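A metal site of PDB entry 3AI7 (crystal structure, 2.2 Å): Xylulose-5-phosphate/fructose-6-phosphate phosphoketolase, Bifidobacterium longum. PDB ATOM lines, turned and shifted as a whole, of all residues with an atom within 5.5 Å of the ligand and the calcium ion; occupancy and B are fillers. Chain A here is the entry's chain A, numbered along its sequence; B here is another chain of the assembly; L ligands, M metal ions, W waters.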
ATOM      1  N   GLY A  66      -4.297 -12.164  20.760  1.00  0.00           N
ATOM      2  CA  GLY A  66      -4.828 -13.584  20.658  1.00  0.00           C
ATOM      3  C   GLY A  66      -5.181 -14.219  21.999  1.00  0.00           C
ATOM      4  O   GLY A  66      -6.368 -14.643  22.239  1.00  0.00           O
ATOM      5  N   THR A  67      -4.199 -14.217  22.909  1.00  0.00           N
ATOM      6  CA  THR A  67      -4.304 -14.973  24.176  1.00  0.00           C
ATOM      7  C   THR A  67      -5.119 -14.109  25.144  1.00  0.00           C
ATOM      8  O   THR A  67      -5.726 -14.571  26.062  1.00  0.00           O
ATOM      9  CB  THR A  67      -2.896 -15.183  24.807  1.00  0.00           C
ATOM     10  OG1 THR A  67      -2.976 -16.185  25.819  1.00  0.00           O
ATOM     11  CG2 THR A  67      -2.278 -13.833  25.391  1.00  0.00           C
ATOM     12  N   PRO A  95       1.237 -17.601  29.001  1.00  0.00           N
ATOM     13  CA  PRO A  95       1.308 -16.773  27.754  1.00  0.00           C
ATOM     14  C   PRO A  95       1.617 -15.351  28.136  1.00  0.00           C
ATOM     15  O   PRO A  95       0.734 -14.480  28.105  1.00  0.00           O
ATOM     16  CB  PRO A  95      -0.120 -16.832  27.165  1.00  0.00           C
ATOM     17  CG  PRO A  95      -0.833 -18.065  27.952  1.00  0.00           C
ATOM     18  CD  PRO A  95      -0.130 -18.090  29.310  1.00  0.00           C
ATOM     19  N   HIS A  97       3.018 -13.095  26.834  1.00  0.00           N
ATOM     20  CA  HIS A  97       2.865 -12.050  25.790  1.00  0.00           C
ATOM     21  C   HIS A  97       1.455 -11.470  25.872  1.00  0.00           C
ATOM     22  O   HIS A  97       1.142 -10.504  25.150  1.00  0.00           O
ATOM     23  CB  HIS A  97       3.093 -12.620  24.388  1.00  0.00           C
ATOM     24  CG  HIS A  97       2.388 -13.939  24.178  1.00  0.00           C
ATOM     25  ND1 HIS A  97       2.851 -15.133  24.729  1.00  0.00           N
ATOM     26  CD2 HIS A  97       1.263 -14.251  23.490  1.00  0.00           C
ATOM     27  CE1 HIS A  97       2.052 -16.125  24.386  1.00  0.00           C
ATOM     28  NE2 HIS A  97       1.050 -15.619  23.663  1.00  0.00           N
ATOM     29  N   GLY A 154       7.033 -14.981  31.303  1.00  0.00           N
ATOM     30  CA  GLY A 154       6.524 -15.703  30.219  1.00  0.00           C
ATOM     31  C   GLY A 154       7.003 -15.262  28.862  1.00  0.00           C
ATOM     32  O   GLY A 154       6.269 -15.438  27.896  1.00  0.00           O
ATOM     33  N   GLY A 155       8.195 -14.688  28.750  1.00  0.00           N
ATOM     34  CA  GLY A 155       8.733 -14.324  27.442  1.00  0.00           C
ATOM     35  C   GLY A 155       9.254 -15.526  26.668  1.00  0.00           C
ATOM     36  O   GLY A 155       8.884 -15.754  25.504  1.00  0.00           O
ATOM     37  N   GLU A 156      10.115 -16.308  27.321  1.00  0.00           N
ATOM     38  CA  GLU A 156      10.525 -17.608  26.823  1.00  0.00           C
ATOM     39  C   GLU A 156       9.578 -18.632  27.445  1.00  0.00           C
ATOM     40  O   GLU A 156       9.580 -18.829  28.691  1.00  0.00           O
ATOM     41  CB  GLU A 156      11.950 -17.931  27.323  1.00  0.00           C
ATOM     42  CG  GLU A 156      12.543 -19.203  26.729  1.00  0.00           C
ATOM     43  CD  GLU A 156      14.054 -19.263  27.005  1.00  0.00           C
ATOM     44  OE1 GLU A 156      14.829 -18.439  26.427  1.00  0.00           O
ATOM     45  OE2 GLU A 156      14.452 -20.115  27.829  1.00  0.00           O
ATOM     46  N   LEU A 157       8.834 -19.325  26.610  1.00  0.00           N
ATOM     47  CA  LEU A 157       7.750 -20.159  27.094  1.00  0.00           C
ATOM     48  C   LEU A 157       8.335 -21.427  27.605  1.00  0.00           C
ATOM     49  O   LEU A 157       9.421 -21.850  27.124  1.00  0.00           O
ATOM     50  CB  LEU A 157       6.841 -20.474  25.933  1.00  0.00           C
ATOM     51  CG  LEU A 157       6.136 -19.218  25.408  1.00  0.00           C
ATOM     52  CD1 LEU A 157       5.325 -19.621  24.124  1.00  0.00           C
ATOM     53  CD2 LEU A 157       5.219 -18.696  26.486  1.00  0.00           C
ATOM     54  N   GLY A 181      -0.052 -21.997  28.040  1.00  0.00           N
ATOM     55  CA  GLY A 181      -0.521 -21.902  26.624  1.00  0.00           C
ATOM     56  C   GLY A 181      -0.617 -23.308  26.043  1.00  0.00           C
ATOM     57  O   GLY A 181       0.141 -24.185  26.435  1.00  0.00           O
ATOM     58  N   ASP A 182      -1.489 -23.523  25.061  1.00  0.00           N
ATOM     59  CA  ASP A 182      -1.460 -24.846  24.420  1.00  0.00           C
ATOM     60  C   ASP A 182      -0.248 -25.021  23.486  1.00  0.00           C
ATOM     61  O   ASP A 182       0.258 -26.181  23.315  1.00  0.00           O
ATOM     62  CB  ASP A 182      -2.812 -25.259  23.809  1.00  0.00           C
ATOM     63  CG  ASP A 182      -3.410 -24.251  22.815  1.00  0.00           C
ATOM     64  OD1 ASP A 182      -2.962 -23.094  22.723  1.00  0.00           O
ATOM     65  OD2 ASP A 182      -4.316 -24.674  22.074  1.00  0.00           O
ATOM     66  N   GLY A 183       0.279 -23.909  22.980  1.00  0.00           N
ATOM     67  CA  GLY A 183       1.558 -23.899  22.207  1.00  0.00           C
ATOM     68  C   GLY A 183       2.669 -24.147  23.217  1.00  0.00           C
ATOM     69  O   GLY A 183       3.501 -25.071  23.026  1.00  0.00           O
ATOM     70  N   GLU A 184       2.701 -23.346  24.286  1.00  0.00           N
ATOM     71  CA  GLU A 184       3.668 -23.542  25.319  1.00  0.00           C
ATOM     72  C   GLU A 184       3.751 -25.037  25.770  1.00  0.00           C
ATOM     73  O   GLU A 184       4.818 -25.561  26.046  1.00  0.00           O
ATOM     74  CB  GLU A 184       3.417 -22.628  26.515  1.00  0.00           C
ATOM     75  CG  GLU A 184       4.312 -22.951  27.745  1.00  0.00           C
ATOM     76  CD  GLU A 184       4.146 -21.955  28.893  1.00  0.00           C
ATOM     77  OE1 GLU A 184       3.028 -21.364  29.029  1.00  0.00           O
ATOM     78  OE2 GLU A 184       5.148 -21.730  29.657  1.00  0.00           O
ATOM     79  N   ALA A 185       2.617 -25.697  25.853  1.00  0.00           N
ATOM     80  CA  ALA A 185       2.614 -27.130  26.279  1.00  0.00           C
ATOM     81  C   ALA A 185       3.329 -28.030  25.315  1.00  0.00           C
ATOM     82  O   ALA A 185       3.625 -29.187  25.678  1.00  0.00           O
ATOM     83  CB  ALA A 185       1.196 -27.660  26.550  1.00  0.00           C
ATOM     84  N   THR A 187       6.454 -27.469  24.405  1.00  0.00           N
ATOM     85  CA  THR A 187       7.862 -27.331  24.751  1.00  0.00           C
ATOM     86  C   THR A 187       8.268 -28.493  25.685  1.00  0.00           C
ATOM     87  O   THR A 187       7.459 -28.990  26.456  1.00  0.00           O
ATOM     88  CB  THR A 187       8.264 -26.009  25.480  1.00  0.00           C
ATOM     89  OG1 THR A 187       7.678 -26.062  26.773  1.00  0.00           O
ATOM     90  CG2 THR A 187       7.808 -24.761  24.792  1.00  0.00           C
ATOM     91  N   HIS A 213      -4.836 -23.430  28.541  1.00  0.00           N
ATOM     92  CA  HIS A 213      -5.481 -22.392  27.777  1.00  0.00           C
ATOM     93  C   HIS A 213      -5.566 -22.899  26.333  1.00  0.00           C
ATOM     94  O   HIS A 213      -4.790 -22.528  25.434  1.00  0.00           O
ATOM     95  CB  HIS A 213      -4.680 -21.091  27.859  1.00  0.00           C
ATOM     96  CG  HIS A 213      -5.404 -19.924  27.248  1.00  0.00           C
ATOM     97  ND1 HIS A 213      -4.847 -18.670  27.168  1.00  0.00           N
ATOM     98  CD2 HIS A 213      -6.592 -19.847  26.625  1.00  0.00           C
ATOM     99  CE1 HIS A 213      -5.687 -17.847  26.545  1.00  0.00           C
ATOM    100  NE2 HIS A 213      -6.763 -18.543  26.213  1.00  0.00           N
ATOM    101  N   ASN A 215      -6.801 -22.614  23.361  1.00  0.00           N
ATOM    102  CA  ASN A 215      -7.426 -21.729  22.382  1.00  0.00           C
ATOM    103  C   ASN A 215      -7.149 -22.140  20.961  1.00  0.00           C
ATOM    104  O   ASN A 215      -7.615 -21.487  19.996  1.00  0.00           O
ATOM    105  CB  ASN A 215      -7.066 -20.264  22.623  1.00  0.00           C
ATOM    106  CG  ASN A 215      -5.619 -20.009  22.484  1.00  0.00           C
ATOM    107  OD1 ASN A 215      -4.896 -20.800  21.875  1.00  0.00           O
ATOM    108  ND2 ASN A 215      -5.157 -18.872  22.992  1.00  0.00           N
ATOM    109  N   GLY A 216      -6.410 -23.247  20.826  1.00  0.00           N
ATOM    110  CA  GLY A 216      -6.377 -23.967  19.527  1.00  0.00           C
ATOM    111  C   GLY A 216      -5.239 -23.631  18.573  1.00  0.00           C
ATOM    112  O   GLY A 216      -5.058 -24.318  17.546  1.00  0.00           O
ATOM    113  N   TYR A 217      -4.535 -22.521  18.844  1.00  0.00           N
ATOM    114  CA  TYR A 217      -3.502 -22.032  17.939  1.00  0.00           C
ATOM    115  C   TYR A 217      -2.329 -21.493  18.651  1.00  0.00           C
ATOM    116  O   TYR A 217      -2.439 -21.035  19.819  1.00  0.00           O
ATOM    117  CB  TYR A 217      -4.075 -20.914  17.030  1.00  0.00           C
ATOM    118  CG  TYR A 217      -5.201 -21.467  16.255  1.00  0.00           C
ATOM    119  CD1 TYR A 217      -4.936 -22.132  15.073  1.00  0.00           C
ATOM    120  CD2 TYR A 217      -6.495 -21.493  16.794  1.00  0.00           C
ATOM    121  CE1 TYR A 217      -5.956 -22.745  14.351  1.00  0.00           C
ATOM    122  CE2 TYR A 217      -7.571 -22.102  16.077  1.00  0.00           C
ATOM    123  CZ  TYR A 217      -7.294 -22.726  14.840  1.00  0.00           C
ATOM    124  OH  TYR A 217      -8.267 -23.386  14.087  1.00  0.00           O
ATOM    125  N   LYS A 218      -1.199 -21.500  17.954  1.00  0.00           N
ATOM    126  CA  LYS A 218       0.011 -20.808  18.410  1.00  0.00           C
ATOM    127  C   LYS A 218       0.216 -19.592  17.418  1.00  0.00           C
ATOM    128  O   LYS A 218      -0.737 -18.883  17.115  1.00  0.00           O
ATOM    129  CB  LYS A 218       1.212 -21.802  18.592  1.00  0.00           C
ATOM    130  CG  LYS A 218       1.348 -23.001  17.624  1.00  0.00           C
ATOM    131  CD  LYS A 218       2.486 -23.932  17.989  1.00  0.00           C
ATOM    132  CE  LYS A 218       2.770 -24.963  16.883  1.00  0.00           C
ATOM    133  NZ  LYS A 218       1.935 -26.179  16.981  1.00  0.00           N
ATOM    134  N   ILE A 219       1.399 -19.370  16.888  1.00  0.00           N
ATOM    135  CA  ILE A 219       1.580 -18.205  16.073  1.00  0.00           C
ATOM    136  C   ILE A 219       0.943 -18.398  14.693  1.00  0.00           C
ATOM    137  O   ILE A 219       0.156 -17.542  14.173  1.00  0.00           O
ATOM    138  CB  ILE A 219       3.052 -17.870  15.846  1.00  0.00           C
ATOM    139  CG1 ILE A 219       3.763 -17.472  17.176  1.00  0.00           C
ATOM    140  CG2 ILE A 219       3.141 -16.690  14.841  1.00  0.00           C
ATOM    141  CD1 ILE A 219       5.285 -17.043  16.969  1.00  0.00           C
ATOM    142  N   THR A 223      -2.508 -26.169  17.444  1.00  0.00           N
ATOM    143  CA  THR A 223      -1.710 -26.780  18.468  1.00  0.00           C
ATOM    144  C   THR A 223      -2.062 -28.248  18.517  1.00  0.00           C
ATOM    145  O   THR A 223      -3.242 -28.632  18.378  1.00  0.00           O
ATOM    146  CB  THR A 223      -2.010 -26.108  19.814  1.00  0.00           C
ATOM    147  OG1 THR A 223      -3.423 -26.045  19.958  1.00  0.00           O
ATOM    148  CG2 THR A 223      -1.486 -24.654  19.799  1.00  0.00           C
ATOM    149  N   LYS A 300      -9.288 -18.573  19.994  1.00  0.00           N
ATOM    150  CA  LYS A 300      -8.234 -17.652  20.249  1.00  0.00           C
ATOM    151  C   LYS A 300      -8.728 -16.296  19.737  1.00  0.00           C
ATOM    152  O   LYS A 300      -9.472 -16.205  18.745  1.00  0.00           O
ATOM    153  CB  LYS A 300      -6.967 -18.106  19.540  1.00  0.00           C
ATOM    154  CG  LYS A 300      -5.832 -17.139  19.637  1.00  0.00           C
ATOM    155  CD  LYS A 300      -4.562 -17.764  19.052  1.00  0.00           C
ATOM    156  CE  LYS A 300      -3.329 -17.005  19.548  1.00  0.00           C
ATOM    157  NZ  LYS A 300      -2.081 -17.865  19.391  1.00  0.00           N
ATOM    158  N   HIS A 320      -3.238 -13.871  16.646  1.00  0.00           N
ATOM    159  CA  HIS A 320      -2.189 -14.040  17.664  1.00  0.00           C
ATOM    160  C   HIS A 320      -1.594 -12.723  18.153  1.00  0.00           C
ATOM    161  O   HIS A 320      -1.454 -12.459  19.326  1.00  0.00           O
ATOM    162  CB  HIS A 320      -1.067 -14.910  17.096  1.00  0.00           C
ATOM    163  CG  HIS A 320       0.096 -15.038  18.003  1.00  0.00           C
ATOM    164  ND1 HIS A 320       0.003 -15.640  19.231  1.00  0.00           N
ATOM    165  CD2 HIS A 320       1.369 -14.567  17.902  1.00  0.00           C
ATOM    166  CE1 HIS A 320       1.167 -15.555  19.848  1.00  0.00           C
ATOM    167  NE2 HIS A 320       2.020 -14.922  19.057  1.00  0.00           N
ATOM    168  N   PRO B 435      10.266 -23.848  15.054  1.00  0.00           N
ATOM    169  CA  PRO B 435       9.381 -23.949  16.206  1.00  0.00           C
ATOM    170  C   PRO B 435       8.234 -22.920  16.102  1.00  0.00           C
ATOM    171  O   PRO B 435       8.127 -22.009  16.936  1.00  0.00           O
ATOM    172  CB  PRO B 435      10.344 -23.680  17.397  1.00  0.00           C
ATOM    173  CG  PRO B 435      11.366 -22.781  16.786  1.00  0.00           C
ATOM    174  CD  PRO B 435      11.390 -22.926  15.305  1.00  0.00           C
ATOM    175  N   ASP B 436       7.405 -23.061  15.066  1.00  0.00           N
ATOM    176  CA  ASP B 436       6.238 -22.201  14.829  1.00  0.00           C
ATOM    177  C   ASP B 436       6.702 -20.846  14.353  1.00  0.00           C
ATOM    178  O   ASP B 436       6.025 -19.851  14.511  1.00  0.00           O
ATOM    179  CB  ASP B 436       5.392 -22.122  16.102  1.00  0.00           C
ATOM    180  CG  ASP B 436       4.044 -21.360  15.941  1.00  0.00           C
ATOM    181  OD1 ASP B 436       3.292 -21.464  14.905  1.00  0.00           O
ATOM    182  OD2 ASP B 436       3.733 -20.645  16.925  1.00  0.00           O
ATOM    183  N   GLU B 437       7.865 -20.807  13.710  1.00  0.00           N
ATOM    184  CA  GLU B 437       8.451 -19.543  13.286  1.00  0.00           C
ATOM    185  C   GLU B 437       8.908 -19.480  11.832  1.00  0.00           C
ATOM    186  O   GLU B 437       9.471 -18.478  11.435  1.00  0.00           O
ATOM    187  CB  GLU B 437       9.656 -19.188  14.175  1.00  0.00           C
ATOM    188  CG  GLU B 437       9.300 -19.036  15.653  1.00  0.00           C
ATOM    189  CD  GLU B 437      10.541 -19.081  16.558  1.00  0.00           C
ATOM    190  OE1 GLU B 437      11.657 -19.012  16.015  1.00  0.00           O
ATOM    191  OE2 GLU B 437      10.414 -19.174  17.802  1.00  0.00           O
ATOM    192  N   LEU B 477       6.164 -26.310  18.742  1.00  0.00           N
ATOM    193  CA  LEU B 477       6.745 -25.212  19.497  1.00  0.00           C
ATOM    194  C   LEU B 477       7.683 -25.850  20.493  1.00  0.00           C
ATOM    195  O   LEU B 477       7.352 -26.025  21.667  1.00  0.00           O
ATOM    196  CB  LEU B 477       5.668 -24.322  20.126  1.00  0.00           C
ATOM    197  CG  LEU B 477       5.923 -23.152  21.080  1.00  0.00           C
ATOM    198  CD1 LEU B 477       7.393 -22.637  21.248  1.00  0.00           C
ATOM    199  CD2 LEU B 477       4.805 -21.991  21.063  1.00  0.00           C
ATOM    200  N   GLU B 479      12.137 -25.904  20.416  1.00  0.00           N
ATOM    201  CA  GLU B 479      13.487 -25.897  19.892  1.00  0.00           C
ATOM    202  C   GLU B 479      14.151 -27.277  20.049  1.00  0.00           C
ATOM    203  O   GLU B 479      14.935 -27.655  19.182  1.00  0.00           O
ATOM    204  CB  GLU B 479      14.347 -24.774  20.558  1.00  0.00           C
ATOM    205  CG  GLU B 479      13.838 -23.340  20.175  1.00  0.00           C
ATOM    206  CD  GLU B 479      12.580 -22.906  20.981  1.00  0.00           C
ATOM    207  OE1 GLU B 479      12.145 -23.659  21.901  1.00  0.00           O
ATOM    208  OE2 GLU B 479      11.960 -21.861  20.626  1.00  0.00           O
ATOM    209  N   TYR B 501      14.204 -17.624  16.461  1.00  0.00           N
ATOM    210  CA  TYR B 501      14.480 -16.347  16.989  1.00  0.00           C
ATOM    211  C   TYR B 501      15.784 -16.553  17.708  1.00  0.00           C
ATOM    212  O   TYR B 501      16.016 -17.596  18.416  1.00  0.00           O
ATOM    213  CB  TYR B 501      13.437 -15.923  18.041  1.00  0.00           C
ATOM    214  CG  TYR B 501      12.068 -15.634  17.470  1.00  0.00           C
ATOM    215  CD1 TYR B 501      11.848 -15.665  16.103  1.00  0.00           C
ATOM    216  CD2 TYR B 501      10.974 -15.360  18.321  1.00  0.00           C
ATOM    217  CE1 TYR B 501      10.546 -15.401  15.542  1.00  0.00           C
ATOM    218  CE2 TYR B 501       9.688 -15.097  17.801  1.00  0.00           C
ATOM    219  CZ  TYR B 501       9.476 -15.130  16.413  1.00  0.00           C
ATOM    220  OH  TYR B 501       8.223 -14.870  15.892  1.00  0.00           O
ATOM    221  N   PHE B 504      16.108 -17.450  21.538  1.00  0.00           N
ATOM    222  CA  PHE B 504      15.700 -18.759  21.990  1.00  0.00           C
ATOM    223  C   PHE B 504      16.562 -19.889  21.428  1.00  0.00           C
ATOM    224  O   PHE B 504      16.320 -21.068  21.781  1.00  0.00           O
ATOM    225  CB  PHE B 504      14.191 -19.029  21.799  1.00  0.00           C
ATOM    226  CG  PHE B 504      13.288 -17.879  22.338  1.00  0.00           C
ATOM    227  CD1 PHE B 504      13.567 -17.267  23.552  1.00  0.00           C
ATOM    228  CD2 PHE B 504      12.221 -17.450  21.618  1.00  0.00           C
ATOM    229  CE1 PHE B 504      12.816 -16.220  24.016  1.00  0.00           C
ATOM    230  CE2 PHE B 504      11.456 -16.357  22.063  1.00  0.00           C
ATOM    231  CZ  PHE B 504      11.732 -15.772  23.267  1.00  0.00           C
ATOM    232  N   VAL B 507      17.848 -22.050  24.026  1.00  0.00           N
ATOM    233  CA  VAL B 507      17.082 -23.153  24.626  1.00  0.00           C
ATOM    234  C   VAL B 507      17.844 -24.503  24.318  1.00  0.00           C
ATOM    235  O   VAL B 507      17.864 -25.415  25.103  1.00  0.00           O
ATOM    236  CB  VAL B 507      15.702 -23.214  24.029  1.00  0.00           C
ATOM    237  CG1 VAL B 507      15.028 -24.619  24.212  1.00  0.00           C
ATOM    238  CG2 VAL B 507      14.791 -22.015  24.538  1.00  0.00           C
ATOM    239  N   HIS B 553      13.582 -11.307  24.836  1.00  0.00           N
ATOM    240  CA  HIS B 553      13.881 -11.783  23.531  1.00  0.00           C
ATOM    241  C   HIS B 553      15.216 -11.224  23.004  1.00  0.00           C
ATOM    242  O   HIS B 553      15.425 -11.236  21.820  1.00  0.00           O
ATOM    243  CB  HIS B 553      12.759 -11.268  22.601  1.00  0.00           C
ATOM    244  CG  HIS B 553      11.474 -12.022  22.719  1.00  0.00           C
ATOM    245  ND1 HIS B 553      10.774 -12.132  23.905  1.00  0.00           N
ATOM    246  CD2 HIS B 553      10.768 -12.712  21.799  1.00  0.00           C
ATOM    247  CE1 HIS B 553       9.682 -12.861  23.695  1.00  0.00           C
ATOM    248  NE2 HIS B 553       9.662 -13.210  22.427  1.00  0.00           N
HETATM  249  N1  LIG L   1      10.065 -20.352  21.650  1.00  0.00           N
HETATM  250  C1  LIG L   1      10.033 -20.139  22.958  1.00  0.00           C
HETATM  251  C2  LIG L   1      10.735 -21.102  23.921  1.00  0.00           C
HETATM  252  N2  LIG L   1       9.379 -19.033  23.440  1.00  0.00           N
HETATM  253  C3  LIG L   1       8.735 -18.176  22.591  1.00  0.00           C
HETATM  254  N3  LIG L   1       8.139 -17.043  23.109  1.00  0.00           N
HETATM  255  C4  LIG L   1       8.767 -18.405  21.221  1.00  0.00           C
HETATM  256  C5  LIG L   1       9.404 -19.541  20.788  1.00  0.00           C
HETATM  257  C6  LIG L   1       8.080 -17.490  20.196  1.00  0.00           C
HETATM  258  N4  LIG L   1       6.626 -17.457  20.547  1.00  0.00           N
HETATM  259  C7  LIG L   1       6.104 -16.400  21.237  1.00  0.00           C
HETATM  260  S1  LIG L   1       4.345 -16.630  21.464  1.00  0.00           S
HETATM  261  C8  LIG L   1       4.409 -18.167  20.540  1.00  0.00           C
HETATM  262  C9  LIG L   1       5.723 -18.414  20.153  1.00  0.00           C
HETATM  263  C10 LIG L   1       6.090 -19.571  19.298  1.00  0.00           C
HETATM  264  C11 LIG L   1       3.090 -18.931  20.368  1.00  0.00           C
HETATM  265  C12 LIG L   1       2.698 -19.484  21.745  1.00  0.00           C
HETATM  266  O1  LIG L   1       1.335 -19.914  21.664  1.00  0.00           O
HETATM  267  P1  LIG L   1       0.483 -20.327  22.971  1.00  0.00           P
HETATM  268  O2  LIG L   1       1.341 -21.029  24.088  1.00  0.00           O
HETATM  269  O3  LIG L   1      -0.772 -21.283  22.357  1.00  0.00           O
HETATM  270  O4  LIG L   1      -0.035 -18.868  23.476  1.00  0.00           O
HETATM  271  P2  LIG L   1      -1.376 -18.117  22.931  1.00  0.00           P
HETATM  272  O5  LIG L   1      -2.118 -18.860  21.804  1.00  0.00           O
HETATM  273  O6  LIG L   1      -2.422 -18.178  24.323  1.00  0.00           O
HETATM  274  O7  LIG L   1      -1.096 -16.525  22.373  1.00  0.00           O
HETATM  275 CA    CA M   1      -2.688 -21.018  22.025  1.00  0.00          CA
HETATM  276  O   HOH W   1      -2.859 -20.723  24.294  1.00  0.00           O
HETATM  277  O   HOH W   2       5.558 -13.074  21.592  1.00  0.00           O
HETATM  278  O   HOH W   3       7.949 -14.358  20.615  1.00  0.00           O
HETATM  279  O   HOH W   4       1.809 -19.588  26.566  1.00  0.00           O
HETATM  280  O   HOH W   5      -1.690 -14.064  21.632  1.00  0.00           O
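Water W1 lies within hydrogen-bond range of O6 of the ligand (2.6 Å), O of His 213 (2.9 Å), N of Asp 182 (3.2 Å) and ND2 of Asn 215 (3.2 Å).
Water W5 lies within hydrogen-bond range of O7 of the ligand, O of His 320, N of Thr 67 and N of Gly 66.
Water W4 lies within hydrogen-bond range of an oxygen (O2) of the ligand (2.9 Å), the side-chain carboxylate of Glu 184 (3.3 Å) and the backbone NH of Gly 181 (3.4 Å).
Merely in contact with the ligand: Pro 95 (3.9 Å), Glu 156 (3.8 Å), Gly 181 (3.3 Å), His 213 (3.8 Å), Lys 218 (3.6 Å), Ile 219 (3.5 Å), Pro 435 of chain B (3.96 Å), Asp 436 of chain B (3.5 Å), Glu 437 of chain B (3.2 Å), Leu 477 of chain B (3.3 Å), Tyr 501 of chain B (3.7 Å) and Phe 504 of chain B (3.3 Å).
Hydrophobic or aromatic side chains within 4 Å of the ligand: Pro 95, His 97, Leu 157, His 213, Ile 219, His 320, Leu 477 of chain B, Tyr 501 of chain B and Phe 504 of chain B.
Within 4 Å of the ligand: Thr 67, Pro 95, His 97, Gly 155, Glu 156, Leu 157, Gly 181, Asp 182, Gly 183, Glu 184, His 213, Asn 215, Tyr 217, Lys 218, Ile 219, Lys 300, His 320, Pro 435 of chain B, Asp 436 of chain B, Glu 437 of chain B, Leu 477 of chain B, Glu 479 of chain B, Tyr 501 of chain B and Phe 504 of chain B.
OG1 of Thr 67 sits at hydrogen-bond distance from O6 of the ligand (2.6 Å).
O7 of the ligand lies within salt-bridge range of NZ of Lys 300.
The side-chain carboxylate (OE2) of Glu 479 of chain B lies within hydrogen-bond range of a nitrogen (N1) of the ligand, 2.6 Å away.
An oxygen (O7) of the ligand lies within hydrogen-bond range of a ring nitrogen (NE2) of His 97.
N of Glu 184 lies within hydrogen-bond range of O2 of the ligand (2.7 Å).
The backbone carbonyl oxygen of Gly 155 is in hydrogen-bond range of a nitrogen (N3) of the ligand, 2.8 Å away.
An oxygen (O2) of the ligand lies within hydrogen-bond range of the backbone NH (N) of Gly 183, at 3.3 Å.
The backbone NH (N) of Leu 157 sits at hydrogen-bond distance from a nitrogen (N2) of the ligand.
An oxygen (O7) of the ligand lies within hydrogen-bond range of a ring nitrogen (ND1) of His 320 (3.4 Å).
The side-chain carboxylate (OD2) of Asp 182 sits at hydrogen-bond distance from the side-chain hydroxyl (OG1) of Thr 223, 2.7 Å away.
The backbone carbonyl oxygen of Tyr 217 sits close to the side-chain amino group of Lys 300 (3.2 Å).
The backbone NH (N) of Lys 300 sits at hydrogen-bond distance from the backbone carbonyl oxygen (O) of Asn 215 (3.4 Å).
NZ of Lys 300 is in hydrogen-bond range of ND1 of His 320 (3.1 Å).
The backbone carbonyl oxygen (O) of Glu 184 is in hydrogen-bond range of the side-chain hydroxyl (OG1) of Thr 187.
The backbone NH (N) of Tyr 501 of chain B sits at hydrogen-bond distance from the side-chain carboxylate (OE1) of Glu 437 of chain B.
The backbone carbonyl oxygen (O) of His 320 sits at hydrogen-bond distance from the backbone NH (N) of Gly 66, 3.2 Å away.
N of Ile 219 lies within hydrogen-bond range of OD2 of Asp 436 of chain B, 2.7 Å away.
The calcium ion is bound by an oxygen (O3) of the ligand (2.0 Å), the side-chain carboxylate (OD1) of Asp 182 (2.2 Å), the backbone carbonyl oxygen (O) of Tyr 217 (2.2 Å), the side-chain amide oxygen (OD1) of Asn 215 (2.2 Å), an oxygen (O5) of the ligand (2.2 Å) and water W1 (2.3 Å).
The calcium ion has six donor atoms within binding distance.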
